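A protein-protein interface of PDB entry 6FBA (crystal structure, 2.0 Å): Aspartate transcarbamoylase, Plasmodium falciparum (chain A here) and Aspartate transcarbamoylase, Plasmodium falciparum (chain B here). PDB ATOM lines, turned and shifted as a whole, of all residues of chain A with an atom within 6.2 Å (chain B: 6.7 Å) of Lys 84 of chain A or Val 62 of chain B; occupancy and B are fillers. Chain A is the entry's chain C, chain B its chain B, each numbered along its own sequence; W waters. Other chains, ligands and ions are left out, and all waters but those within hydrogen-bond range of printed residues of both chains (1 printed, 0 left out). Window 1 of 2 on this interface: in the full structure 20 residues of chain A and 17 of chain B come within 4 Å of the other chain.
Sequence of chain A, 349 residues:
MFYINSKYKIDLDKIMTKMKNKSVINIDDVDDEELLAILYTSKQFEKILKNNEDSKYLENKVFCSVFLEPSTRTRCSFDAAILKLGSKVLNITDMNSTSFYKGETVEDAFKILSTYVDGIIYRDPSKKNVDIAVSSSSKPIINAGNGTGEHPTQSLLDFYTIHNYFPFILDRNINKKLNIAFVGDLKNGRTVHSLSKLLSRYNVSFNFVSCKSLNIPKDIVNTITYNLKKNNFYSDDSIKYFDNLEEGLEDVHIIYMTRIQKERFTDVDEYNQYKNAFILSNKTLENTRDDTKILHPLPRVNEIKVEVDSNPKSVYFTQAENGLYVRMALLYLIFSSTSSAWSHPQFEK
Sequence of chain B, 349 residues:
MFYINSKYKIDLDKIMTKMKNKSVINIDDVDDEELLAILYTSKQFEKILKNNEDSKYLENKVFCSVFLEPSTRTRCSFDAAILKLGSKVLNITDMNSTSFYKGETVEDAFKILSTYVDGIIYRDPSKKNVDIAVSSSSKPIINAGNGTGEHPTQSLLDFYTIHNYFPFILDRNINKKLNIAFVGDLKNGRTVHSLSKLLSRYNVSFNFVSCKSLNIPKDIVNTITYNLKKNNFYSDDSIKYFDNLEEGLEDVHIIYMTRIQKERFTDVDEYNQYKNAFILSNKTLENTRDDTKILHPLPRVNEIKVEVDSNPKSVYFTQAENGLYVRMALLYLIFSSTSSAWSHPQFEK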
ATOM      1  N   LEU A  49     -17.166  13.065  -0.058  1.00  0.00           N
ATOM      2  CA  LEU A  49     -16.698  13.246   1.324  1.00  0.00           C
ATOM      3  C   LEU A  49     -15.822  12.097   1.813  1.00  0.00           C
ATOM      4  O   LEU A  49     -14.833  12.347   2.428  1.00  0.00           O
ATOM      5  CB  LEU A  49     -17.854  13.511   2.270  1.00  0.00           C
ATOM      6  CG  LEU A  49     -18.118  15.012   2.415  1.00  0.00           C
ATOM      7  CD1 LEU A  49     -18.239  15.684   1.068  1.00  0.00           C
ATOM      8  CD2 LEU A  49     -19.359  15.331   3.197  1.00  0.00           C
ATOM      9  N   GLU A  53     -12.536  14.477  -1.191  1.00  0.00           N
ATOM     10  CA  GLU A  53     -12.510  15.333  -2.356  1.00  0.00           C
ATOM     11  C   GLU A  53     -13.128  16.715  -2.030  1.00  0.00           C
ATOM     12  O   GLU A  53     -13.753  16.894  -1.008  1.00  0.00           O
ATOM     13  CB  GLU A  53     -13.163  14.677  -3.571  1.00  0.00           C
ATOM     14  CG  GLU A  53     -12.378  13.486  -4.082  1.00  0.00           C
ATOM     15  CD  GLU A  53     -13.212  12.553  -4.943  1.00  0.00           C
ATOM     16  OE1 GLU A  53     -12.836  11.373  -5.028  1.00  0.00           O
ATOM     17  OE2 GLU A  53     -14.235  13.027  -5.509  1.00  0.00           O
ATOM     18  N   ASP A  54     -12.964  17.656  -2.922  1.00  0.00           N
ATOM     19  CA  ASP A  54     -13.413  18.978  -2.798  1.00  0.00           C
ATOM     20  C   ASP A  54     -14.959  18.972  -2.904  1.00  0.00           C
ATOM     21  O   ASP A  54     -15.527  18.479  -3.868  1.00  0.00           O
ATOM     22  CB  ASP A  54     -12.841  19.672  -3.941  1.00  0.00           C
ATOM     23  CG  ASP A  54     -13.177  21.162  -3.970  1.00  0.00           C
ATOM     24  OD1 ASP A  54     -14.094  21.694  -3.339  1.00  0.00           O
ATOM     25  OD2 ASP A  54     -12.458  21.793  -4.728  1.00  0.00           O
ATOM     26  N   SER A  55     -15.648  19.386  -1.855  1.00  0.00           N
ATOM     27  CA  SER A  55     -17.094  19.374  -1.862  1.00  0.00           C
ATOM     28  C   SER A  55     -17.738  20.737  -2.105  1.00  0.00           C
ATOM     29  O   SER A  55     -18.967  20.860  -1.872  1.00  0.00           O
ATOM     30  CB  SER A  55     -17.652  18.769  -0.564  1.00  0.00           C
ATOM     31  OG  SER A  55     -17.328  19.658   0.464  1.00  0.00           O
ATOM     32  N   LYS A  56     -17.002  21.713  -2.603  1.00  0.00           N
ATOM     33  CA  LYS A  56     -17.524  23.087  -2.639  1.00  0.00           C
ATOM     34  C   LYS A  56     -18.319  23.323  -3.920  1.00  0.00           C
ATOM     35  O   LYS A  56     -17.890  23.923  -4.855  1.00  0.00           O
ATOM     36  CB  LYS A  56     -16.398  24.066  -2.533  1.00  0.00           C
ATOM     37  CG  LYS A  56     -15.805  24.087  -1.129  1.00  0.00           C
ATOM     38  CD  LYS A  56     -14.737  25.220  -1.096  1.00  0.00           C
ATOM     39  CE  LYS A  56     -14.507  25.591   0.365  1.00  0.00           C
ATOM     40  NZ  LYS A  56     -13.765  26.817   0.322  1.00  0.00           N
ATOM     41  N   TYR A  57     -19.464  22.720  -3.985  1.00  0.00           N
ATOM     42  CA  TYR A  57     -20.264  22.744  -5.233  1.00  0.00           C
ATOM     43  C   TYR A  57     -21.286  23.845  -5.210  1.00  0.00           C
ATOM     44  O   TYR A  57     -22.001  23.962  -6.085  1.00  0.00           O
ATOM     45  CB  TYR A  57     -20.937  21.415  -5.452  1.00  0.00           C
ATOM     46  CG  TYR A  57     -20.042  20.442  -6.035  1.00  0.00           C
ATOM     47  CD1 TYR A  57     -19.215  19.672  -5.241  1.00  0.00           C
ATOM     48  CD2 TYR A  57     -20.013  20.233  -7.402  1.00  0.00           C
ATOM     49  CE1 TYR A  57     -18.401  18.729  -5.785  1.00  0.00           C
ATOM     50  CE2 TYR A  57     -19.207  19.259  -7.953  1.00  0.00           C
ATOM     51  CZ  TYR A  57     -18.427  18.511  -7.140  1.00  0.00           C
ATOM     52  OH  TYR A  57     -17.582  17.583  -7.655  1.00  0.00           O
ATOM     53  N   ASP A  79     -26.229  23.758   9.111  1.00  0.00           N
ATOM     54  CA  ASP A  79     -25.022  24.632   9.008  1.00  0.00           C
ATOM     55  C   ASP A  79     -23.809  23.837   8.443  1.00  0.00           C
ATOM     56  O   ASP A  79     -23.169  24.308   7.536  1.00  0.00           O
ATOM     57  CB  ASP A  79     -24.619  25.269  10.346  1.00  0.00           C
ATOM     58  CG  ASP A  79     -25.541  26.453  10.847  1.00  0.00           C
ATOM     59  OD1 ASP A  79     -26.501  26.855  10.127  1.00  0.00           O
ATOM     60  OD2 ASP A  79     -25.297  26.861  12.087  1.00  0.00           O
ATOM     61  N   ALA A  80     -23.530  22.629   8.969  1.00  0.00           N
ATOM     62  CA  ALA A  80     -22.482  21.847   8.440  1.00  0.00           C
ATOM     63  C   ALA A  80     -22.639  21.595   6.921  1.00  0.00           C
ATOM     64  O   ALA A  80     -21.654  21.756   6.160  1.00  0.00           O
ATOM     65  CB  ALA A  80     -22.385  20.532   9.176  1.00  0.00           C
ATOM     66  N   ALA A  81     -23.871  21.249   6.455  1.00  0.00           N
ATOM     67  CA  ALA A  81     -24.056  21.040   5.048  1.00  0.00           C
ATOM     68  C   ALA A  81     -23.845  22.283   4.212  1.00  0.00           C
ATOM     69  O   ALA A  81     -23.177  22.236   3.210  1.00  0.00           O
ATOM     70  CB  ALA A  81     -25.432  20.461   4.783  1.00  0.00           C
ATOM     71  N   ILE A  82     -24.336  23.436   4.659  1.00  0.00           N
ATOM     72  CA  ILE A  82     -24.141  24.723   3.942  1.00  0.00           C
ATOM     73  C   ILE A  82     -22.686  25.041   3.843  1.00  0.00           C
ATOM     74  O   ILE A  82     -22.130  25.381   2.752  1.00  0.00           O
ATOM     75  CB  ILE A  82     -24.950  25.887   4.651  1.00  0.00           C
ATOM     76  CG1 ILE A  82     -26.436  25.648   4.516  1.00  0.00           C
ATOM     77  CG2 ILE A  82     -24.602  27.258   4.083  1.00  0.00           C
ATOM     78  CD1 ILE A  82     -27.258  26.434   5.565  1.00  0.00           C
ATOM     79  N   LEU A  83     -21.992  24.962   4.972  1.00  0.00           N
ATOM     80  CA  LEU A  83     -20.590  25.385   4.975  1.00  0.00           C
ATOM     81  C   LEU A  83     -19.714  24.392   4.221  1.00  0.00           C
ATOM     82  O   LEU A  83     -18.858  24.828   3.531  1.00  0.00           O
ATOM     83  CB  LEU A  83     -20.110  25.509   6.453  1.00  0.00           C
ATOM     84  CG  LEU A  83     -20.867  26.529   7.296  1.00  0.00           C
ATOM     85  CD1 LEU A  83     -20.527  26.406   8.743  1.00  0.00           C
ATOM     86  CD2 LEU A  83     -20.630  27.928   6.755  1.00  0.00           C
ATOM     87  N   LYS A  84     -19.984  23.058   4.310  1.00  0.00           N
ATOM     88  CA  LYS A  84     -19.262  22.077   3.507  1.00  0.00           C
ATOM     89  C   LYS A  84     -19.458  22.232   2.009  1.00  0.00           C
ATOM     90  O   LYS A  84     -18.588  21.878   1.224  1.00  0.00           O
ATOM     91  CB  LYS A  84     -19.692  20.650   3.841  1.00  0.00           C
ATOM     92  CG  LYS A  84     -19.055  20.037   5.034  1.00  0.00           C
ATOM     93  CD  LYS A  84     -17.611  19.801   4.825  1.00  0.00           C
ATOM     94  CE  LYS A  84     -17.292  18.716   3.786  1.00  0.00           C
ATOM     95  NZ  LYS A  84     -15.990  18.941   3.053  1.00  0.00           N
ATOM     96  N   LEU A  85     -20.608  22.786   1.602  1.00  0.00           N
ATOM     97  CA  LEU A  85     -20.855  23.149   0.183  1.00  0.00           C
ATOM     98  C   LEU A  85     -20.077  24.362  -0.246  1.00  0.00           C
ATOM     99  O   LEU A  85     -20.029  24.681  -1.403  1.00  0.00           O
ATOM    100  CB  LEU A  85     -22.303  23.331  -0.068  1.00  0.00           C
ATOM    101  CG  LEU A  85     -23.147  21.995  -0.226  1.00  0.00           C
ATOM    102  CD1 LEU A  85     -24.647  22.352  -0.158  1.00  0.00           C
ATOM    103  CD2 LEU A  85     -22.840  21.286  -1.515  1.00  0.00           C
ATOM    104  N   GLY A  86     -19.469  25.071   0.680  1.00  0.00           N
ATOM    105  CA  GLY A  86     -18.658  26.299   0.409  1.00  0.00           C
ATOM    106  C   GLY A  86     -19.487  27.588   0.577  1.00  0.00           C
ATOM    107  O   GLY A  86     -18.984  28.640   0.339  1.00  0.00           O
ATOM    108  N   SER A  87     -20.763  27.463   0.930  1.00  0.00           N
ATOM    109  CA  SER A  87     -21.624  28.626   1.211  1.00  0.00           C
ATOM    110  C   SER A  87     -21.475  29.238   2.616  1.00  0.00           C
ATOM    111  O   SER A  87     -20.614  28.828   3.365  1.00  0.00           O
ATOM    112  CB  SER A  87     -23.110  28.236   0.762  1.00  0.00           C
ATOM    113  OG  SER A  87     -23.019  28.375  -0.686  1.00  0.00           O
ATOM    114  N   LEU A 324     -25.734  14.409   6.440  1.00  0.00           N
ATOM    115  CA  LEU A 324     -24.906  15.459   5.857  1.00  0.00           C
ATOM    116  C   LEU A 324     -25.012  15.380   4.340  1.00  0.00           C
ATOM    117  O   LEU A 324     -25.272  16.409   3.652  1.00  0.00           O
ATOM    118  CB  LEU A 324     -23.448  15.334   6.334  1.00  0.00           C
ATOM    119  CG  LEU A 324     -22.429  16.217   5.685  1.00  0.00           C
ATOM    120  CD1 LEU A 324     -22.709  17.641   6.151  1.00  0.00           C
ATOM    121  CD2 LEU A 324     -21.011  15.758   6.110  1.00  0.00           C
ATOM    122  N   MET A 328     -26.735  18.261   1.944  1.00  0.00           N
ATOM    123  CA  MET A 328     -25.912  18.885   0.928  1.00  0.00           C
ATOM    124  C   MET A 328     -26.565  18.714  -0.428  1.00  0.00           C
ATOM    125  O   MET A 328     -26.581  19.672  -1.233  1.00  0.00           O
ATOM    126  CB  MET A 328     -24.498  18.296   0.933  1.00  0.00           C
ATOM    127  CG  MET A 328     -23.691  18.656   2.109  1.00  0.00           C
ATOM    128  SD  MET A 328     -22.065  17.881   2.231  1.00  0.00           S
ATOM    129  CE  MET A 328     -21.304  18.749   0.888  1.00  0.00           C
ATOM    130  N   GLU B  59      -8.177  26.027   3.826  1.00  0.00           N
ATOM    131  CA  GLU B  59      -9.393  26.456   3.133  1.00  0.00           C
ATOM    132  C   GLU B  59     -10.703  25.650   3.001  1.00  0.00           C
ATOM    133  O   GLU B  59     -11.790  26.268   2.678  1.00  0.00           O
ATOM    134  CB  GLU B  59      -9.040  26.716   1.670  1.00  0.00           C
ATOM    135  CG  GLU B  59      -8.079  27.832   1.462  1.00  0.00           C
ATOM    136  CD  GLU B  59      -7.789  27.964  -0.020  1.00  0.00           C
ATOM    137  OE1 GLU B  59      -6.756  27.422  -0.500  1.00  0.00           O
ATOM    138  OE2 GLU B  59      -8.645  28.564  -0.694  1.00  0.00           O
ATOM    139  N   ASN B  60     -10.608  24.331   3.046  1.00  0.00           N
ATOM    140  CA  ASN B  60     -11.670  23.524   2.744  1.00  0.00           C
ATOM    141  C   ASN B  60     -12.086  22.903   4.041  1.00  0.00           C
ATOM    142  O   ASN B  60     -12.681  21.845   4.014  1.00  0.00           O
ATOM    143  CB  ASN B  60     -11.231  22.442   1.731  1.00  0.00           C
ATOM    144  CG  ASN B  60     -11.218  22.936   0.257  1.00  0.00           C
ATOM    145  OD1 ASN B  60     -12.206  22.667  -0.569  1.00  0.00           O
ATOM    146  ND2 ASN B  60     -10.101  23.570  -0.129  1.00  0.00           N
ATOM    147  N   LYS B  61     -11.796  23.478   5.173  1.00  0.00           N
ATOM    148  CA  LYS B  61     -12.133  22.841   6.418  1.00  0.00           C
ATOM    149  C   LYS B  61     -13.326  23.546   7.050  1.00  0.00           C
ATOM    150  O   LYS B  61     -13.449  24.752   6.965  1.00  0.00           O
ATOM    151  CB  LYS B  61     -10.941  22.851   7.434  1.00  0.00           C
ATOM    152  CG  LYS B  61      -9.701  22.008   7.078  1.00  0.00           C
ATOM    153  CD  LYS B  61     -10.035  20.640   6.559  1.00  0.00           C
ATOM    154  CE  LYS B  61      -8.767  20.036   6.021  1.00  0.00           C
ATOM    155  NZ  LYS B  61      -8.872  18.592   5.877  1.00  0.00           N
ATOM    156  N   VAL B  62     -14.146  22.753   7.728  1.00  0.00           N
ATOM    157  CA  VAL B  62     -15.277  23.209   8.521  1.00  0.00           C
ATOM    158  C   VAL B  62     -15.139  22.706   9.966  1.00  0.00           C
ATOM    159  O   VAL B  62     -15.047  21.495  10.206  1.00  0.00           O
ATOM    160  CB  VAL B  62     -16.604  22.705   7.891  1.00  0.00           C
ATOM    161  CG1 VAL B  62     -17.746  23.191   8.711  1.00  0.00           C
ATOM    162  CG2 VAL B  62     -16.737  23.146   6.464  1.00  0.00           C
ATOM    163  N   PHE B  63     -15.083  23.611  10.902  1.00  0.00           N
ATOM    164  CA  PHE B  63     -15.011  23.333  12.322  1.00  0.00           C
ATOM    165  C   PHE B  63     -16.295  23.556  13.089  1.00  0.00           C
ATOM    166  O   PHE B  63     -17.193  24.291  12.633  1.00  0.00           O
ATOM    167  CB  PHE B  63     -13.964  24.271  12.947  1.00  0.00           C
ATOM    168  CG  PHE B  63     -12.563  24.014  12.421  1.00  0.00           C
ATOM    169  CD1 PHE B  63     -11.766  23.034  12.981  1.00  0.00           C
ATOM    170  CD2 PHE B  63     -12.073  24.668  11.338  1.00  0.00           C
ATOM    171  CE1 PHE B  63     -10.464  22.787  12.493  1.00  0.00           C
ATOM    172  CE2 PHE B  63     -10.852  24.411  10.816  1.00  0.00           C
ATOM    173  CZ  PHE B  63     -10.041  23.446  11.353  1.00  0.00           C
ATOM    174  N   CYS B  64     -16.401  22.903  14.251  1.00  0.00           N
ATOM    175  CA  CYS B  64     -17.467  23.212  15.184  1.00  0.00           C
ATOM    176  C   CYS B  64     -16.847  23.672  16.466  1.00  0.00           C
ATOM    177  O   CYS B  64     -15.988  23.037  16.992  1.00  0.00           O
ATOM    178  CB  CYS B  64     -18.480  22.057  15.394  1.00  0.00           C
ATOM    179  SG  CYS B  64     -19.772  22.430  16.612  1.00  0.00           S
ATOM    180  N   ILE B  82      -9.644  30.533  12.928  1.00  0.00           N
ATOM    181  CA  ILE B  82     -10.204  29.627  11.900  1.00  0.00           C
ATOM    182  C   ILE B  82     -10.501  30.373  10.612  1.00  0.00           C
ATOM    183  O   ILE B  82     -10.164  29.940   9.491  1.00  0.00           O
ATOM    184  CB  ILE B  82     -11.493  28.939  12.454  1.00  0.00           C
ATOM    185  CG1 ILE B  82     -11.179  27.972  13.564  1.00  0.00           C
ATOM    186  CG2 ILE B  82     -12.305  28.210  11.367  1.00  0.00           C
ATOM    187  CD1 ILE B  82     -12.381  27.653  14.466  1.00  0.00           C
ATOM    188  N   SER B  87     -11.007  28.906   6.577  1.00  0.00           N
ATOM    189  CA  SER B  87     -11.924  27.902   6.967  1.00  0.00           C
ATOM    190  C   SER B  87     -13.264  28.506   7.519  1.00  0.00           C
ATOM    191  O   SER B  87     -13.410  29.753   7.596  1.00  0.00           O
ATOM    192  CB  SER B  87     -11.221  26.948   7.997  1.00  0.00           C
ATOM    193  OG  SER B  87     -10.540  25.998   7.090  1.00  0.00           O
ATOM    194  N   LYS B  88     -14.187  27.606   7.873  1.00  0.00           N
ATOM    195  CA  LYS B  88     -15.492  28.001   8.323  1.00  0.00           C
ATOM    196  C   LYS B  88     -15.704  27.337   9.656  1.00  0.00           C
ATOM    197  O   LYS B  88     -15.159  26.306   9.998  1.00  0.00           O
ATOM    198  CB  LYS B  88     -16.593  27.601   7.287  1.00  0.00           C
ATOM    199  CG  LYS B  88     -16.424  28.233   5.956  1.00  0.00           C
ATOM    200  CD  LYS B  88     -17.195  27.462   4.959  1.00  0.00           C
ATOM    201  CE  LYS B  88     -17.080  28.051   3.576  1.00  0.00           C
ATOM    202  NZ  LYS B  88     -17.766  29.449   3.404  1.00  0.00           N
ATOM    203  N   VAL B  89     -16.602  27.920  10.400  1.00  0.00           N
ATOM    204  CA  VAL B  89     -16.935  27.446  11.708  1.00  0.00           C
ATOM    205  C   VAL B  89     -18.447  27.592  11.991  1.00  0.00           C
ATOM    206  O   VAL B  89     -19.079  28.579  11.561  1.00  0.00           O
ATOM    207  CB  VAL B  89     -16.128  28.176  12.778  1.00  0.00           C
ATOM    208  CG1 VAL B  89     -16.425  29.666  12.843  1.00  0.00           C
ATOM    209  CG2 VAL B  89     -16.394  27.541  14.134  1.00  0.00           C
ATOM    210  N   LEU B  90     -19.003  26.545  12.593  1.00  0.00           N
ATOM    211  CA  LEU B  90     -20.324  26.671  13.205  1.00  0.00           C
ATOM    212  C   LEU B  90     -20.221  26.563  14.703  1.00  0.00           C
ATOM    213  O   LEU B  90     -19.339  25.877  15.252  1.00  0.00           O
ATOM    214  CB  LEU B  90     -21.377  25.672  12.651  1.00  0.00           C
ATOM    215  CG  LEU B  90     -20.958  24.239  12.820  1.00  0.00           C
ATOM    216  CD1 LEU B  90     -22.028  23.432  13.547  1.00  0.00           C
ATOM    217  CD2 LEU B  90     -20.705  23.661  11.450  1.00  0.00           C
ATOM    218  N   TYR B 116     -19.888  15.281  11.082  1.00  0.00           N
ATOM    219  CA  TYR B 116     -20.325  16.479  10.351  1.00  0.00           C
ATOM    220  C   TYR B 116     -19.246  17.482  10.049  1.00  0.00           C
ATOM    221  O   TYR B 116     -19.474  18.313   9.130  1.00  0.00           O
ATOM    222  CB  TYR B 116     -21.469  17.199  11.156  1.00  0.00           C
ATOM    223  CG  TYR B 116     -22.806  16.499  11.188  1.00  0.00           C
ATOM    224  CD1 TYR B 116     -23.083  15.544  10.282  1.00  0.00           C
ATOM    225  CD2 TYR B 116     -23.819  16.821  12.119  1.00  0.00           C
ATOM    226  CE1 TYR B 116     -24.305  14.846  10.262  1.00  0.00           C
ATOM    227  CE2 TYR B 116     -25.065  16.152  12.096  1.00  0.00           C
ATOM    228  CZ  TYR B 116     -25.305  15.147  11.123  1.00  0.00           C
ATOM    229  OH  TYR B 116     -26.475  14.373  10.851  1.00  0.00           O
ATOM    230  N   VAL B 117     -18.120  17.431  10.787  1.00  0.00           N
ATOM    231  CA  VAL B 117     -17.134  18.497  10.772  1.00  0.00           C
ATOM    232  C   VAL B 117     -15.700  17.858  10.799  1.00  0.00           C
ATOM    233  O   VAL B 117     -15.521  16.645  11.044  1.00  0.00           O
ATOM    234  CB  VAL B 117     -17.299  19.542  11.946  1.00  0.00           C
ATOM    235  CG1 VAL B 117     -18.610  20.345  11.870  1.00  0.00           C
ATOM    236  CG2 VAL B 117     -17.132  18.924  13.308  1.00  0.00           C
ATOM    237  N   ASP B 118     -14.687  18.671  10.541  1.00  0.00           N
ATOM    238  CA  ASP B 118     -13.294  18.198  10.418  1.00  0.00           C
ATOM    239  C   ASP B 118     -12.536  18.319  11.732  1.00  0.00           C
ATOM    240  O   ASP B 118     -11.538  17.658  11.981  1.00  0.00           O
ATOM    241  CB  ASP B 118     -12.564  19.015   9.408  1.00  0.00           C
ATOM    242  CG  ASP B 118     -13.224  19.002   8.043  1.00  0.00           C
ATOM    243  OD1 ASP B 118     -13.434  17.922   7.585  1.00  0.00           O
ATOM    244  OD2 ASP B 118     -13.567  19.993   7.404  1.00  0.00           O
ATOM    245  N   GLY B 119     -13.024  19.172  12.597  1.00  0.00           N
ATOM    246  CA  GLY B 119     -12.494  19.266  13.933  1.00  0.00           C
ATOM    247  C   GLY B 119     -13.408  20.052  14.835  1.00  0.00           C
ATOM    248  O   GLY B 119     -14.321  20.765  14.389  1.00  0.00           O
ATOM    249  N   ILE B 120     -13.134  19.926  16.108  1.00  0.00           N
ATOM    250  CA  ILE B 120     -13.904  20.529  17.138  1.00  0.00           C
ATOM    251  C   ILE B 120     -13.081  21.306  18.180  1.00  0.00           C
ATOM    252  O   ILE B 120     -12.119  20.754  18.762  1.00  0.00           O
ATOM    253  CB  ILE B 120     -14.705  19.454  17.890  1.00  0.00           C
ATOM    254  CG1 ILE B 120     -15.520  18.593  16.880  1.00  0.00           C
ATOM    255  CG2 ILE B 120     -15.622  20.089  18.974  1.00  0.00           C
ATOM    256  CD1 ILE B 120     -15.951  17.322  17.420  1.00  0.00           C
HETATM  257  O   HOH W   1     -13.910  20.655   0.185  1.00  0.00           O
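Water W1 lies within hydrogen-bond range of the side-chain amide oxygen of Asn 60 of chain B (2.7 Å) and the backbone NH of Ser 55 of chain A (3.0 Å).
Of the 16 printed residues of chain B, 7 touch a printed residue of chain A. Printed residues of chain B that touch a printed residue of chain A: Glu 59, Asn 60, Val 62, Lys 88, Val 89, Leu 90 and Tyr 116. Hydrophobic or aromatic side chains of chain A within 4 Å of the printed part of chain B: Ala 80, Leu 83 and Leu 324. Among the printed residues, 14 pairs touch across the chains. Among the printed residues, no Asp or Glu carboxylate lies within 4 Å of a Lys or Arg side-chain nitrogen of the other chain.
OD1 of Asp 54 of chain A sits close to OD1 of Asn 60 of chain B, 3.5 Å away. The side-chain amino group (NZ) of Lys 88 of chain B lies within hydrogen-bond range of the backbone carbonyl oxygen (O) of Gly 86 of chain A. The side-chain amino group (NZ) of Lys 56 of chain A lies within hydrogen-bond range of the backbone carbonyl oxygen (O) of Glu 59 of chain B, at 3.1 Å. NZ of Lys 88 of chain B lies within hydrogen-bond range of O of Ser 87 of chain A, 2.9 Å away.
The backbone NH (N) of Ser 87 of chain A lies within hydrogen-bond range of the backbone carbonyl oxygen (O) of Ile 82 of chain A, 3.1 Å away. N of Phe 63 of chain B sits at hydrogen-bond distance from O of Lys 88 of chain B. The backbone carbonyl oxygen (O) of Lys 84 of chain A is in hydrogen-bond range of the side-chain hydroxyl (OG) of Ser 55 of chain A, 2.7 Å away. The backbone NH (N) of Leu 90 of chain B is in hydrogen-bond range of the backbone carbonyl oxygen (O) of Phe 63 of chain B. The backbone carbonyl oxygen (O) of Leu 90 of chain B lies close to the side-chain sulfur (SG) of Cys 64 of chain B, at 3.7 Å. The backbone carbonyl oxygen of Lys 61 of chain B lies within hydrogen-bond range of the backbone NH of Lys 88 of chain B (3.1 Å).
Of the printed residues of chain B, Lys 84 of chain A touches Val 62. Val 62 of chain B touches just these residues of chain A: Leu 83 and Lys 84. Printed residues of chain A within 4 Å of Asn 60 of chain B: Asp 54 and Lys 56. Of the printed residues of chain B, Ser 87 of chain A touches Lys 88 (2.9 Å). Gly 119 of chain B touches none of the printed residues of chain A. The nearest residue of chain A that does not touch Val 62 of chain B is Ala 80 of chain A (4.9 Å). The nearest printed residue of chain B that does not touch Leu 83 of chain A is Phe 63 of chain B (5.5 Å).
Among the printed residues, merely in contact across the chains: Lys 56 of chain A with Asn 60 of chain B (3.6 Å), Asp 79 of chain A with Leu 90 of chain B (3.998 Å), Ala 80 of chain A with Leu 90 of chain B (3.9 Å), Ala 80 of chain A with Tyr 116 of chain B (3.7 Å), Leu 83 of chain A with Val 62 of chain B (3.9 Å), Leu 83 of chain A with Lys 88 of chain B (3.4 Å), Leu 83 of chain A with Val 89 of chain B (3.8 Å), Leu 83 of chain A with Leu 90 of chain B (3.9 Å), Lys 84 of chain A with Val 62 of chain B (3.8 Å) and Leu 324 of chain A with Tyr 116 of chain B (3.97 Å).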
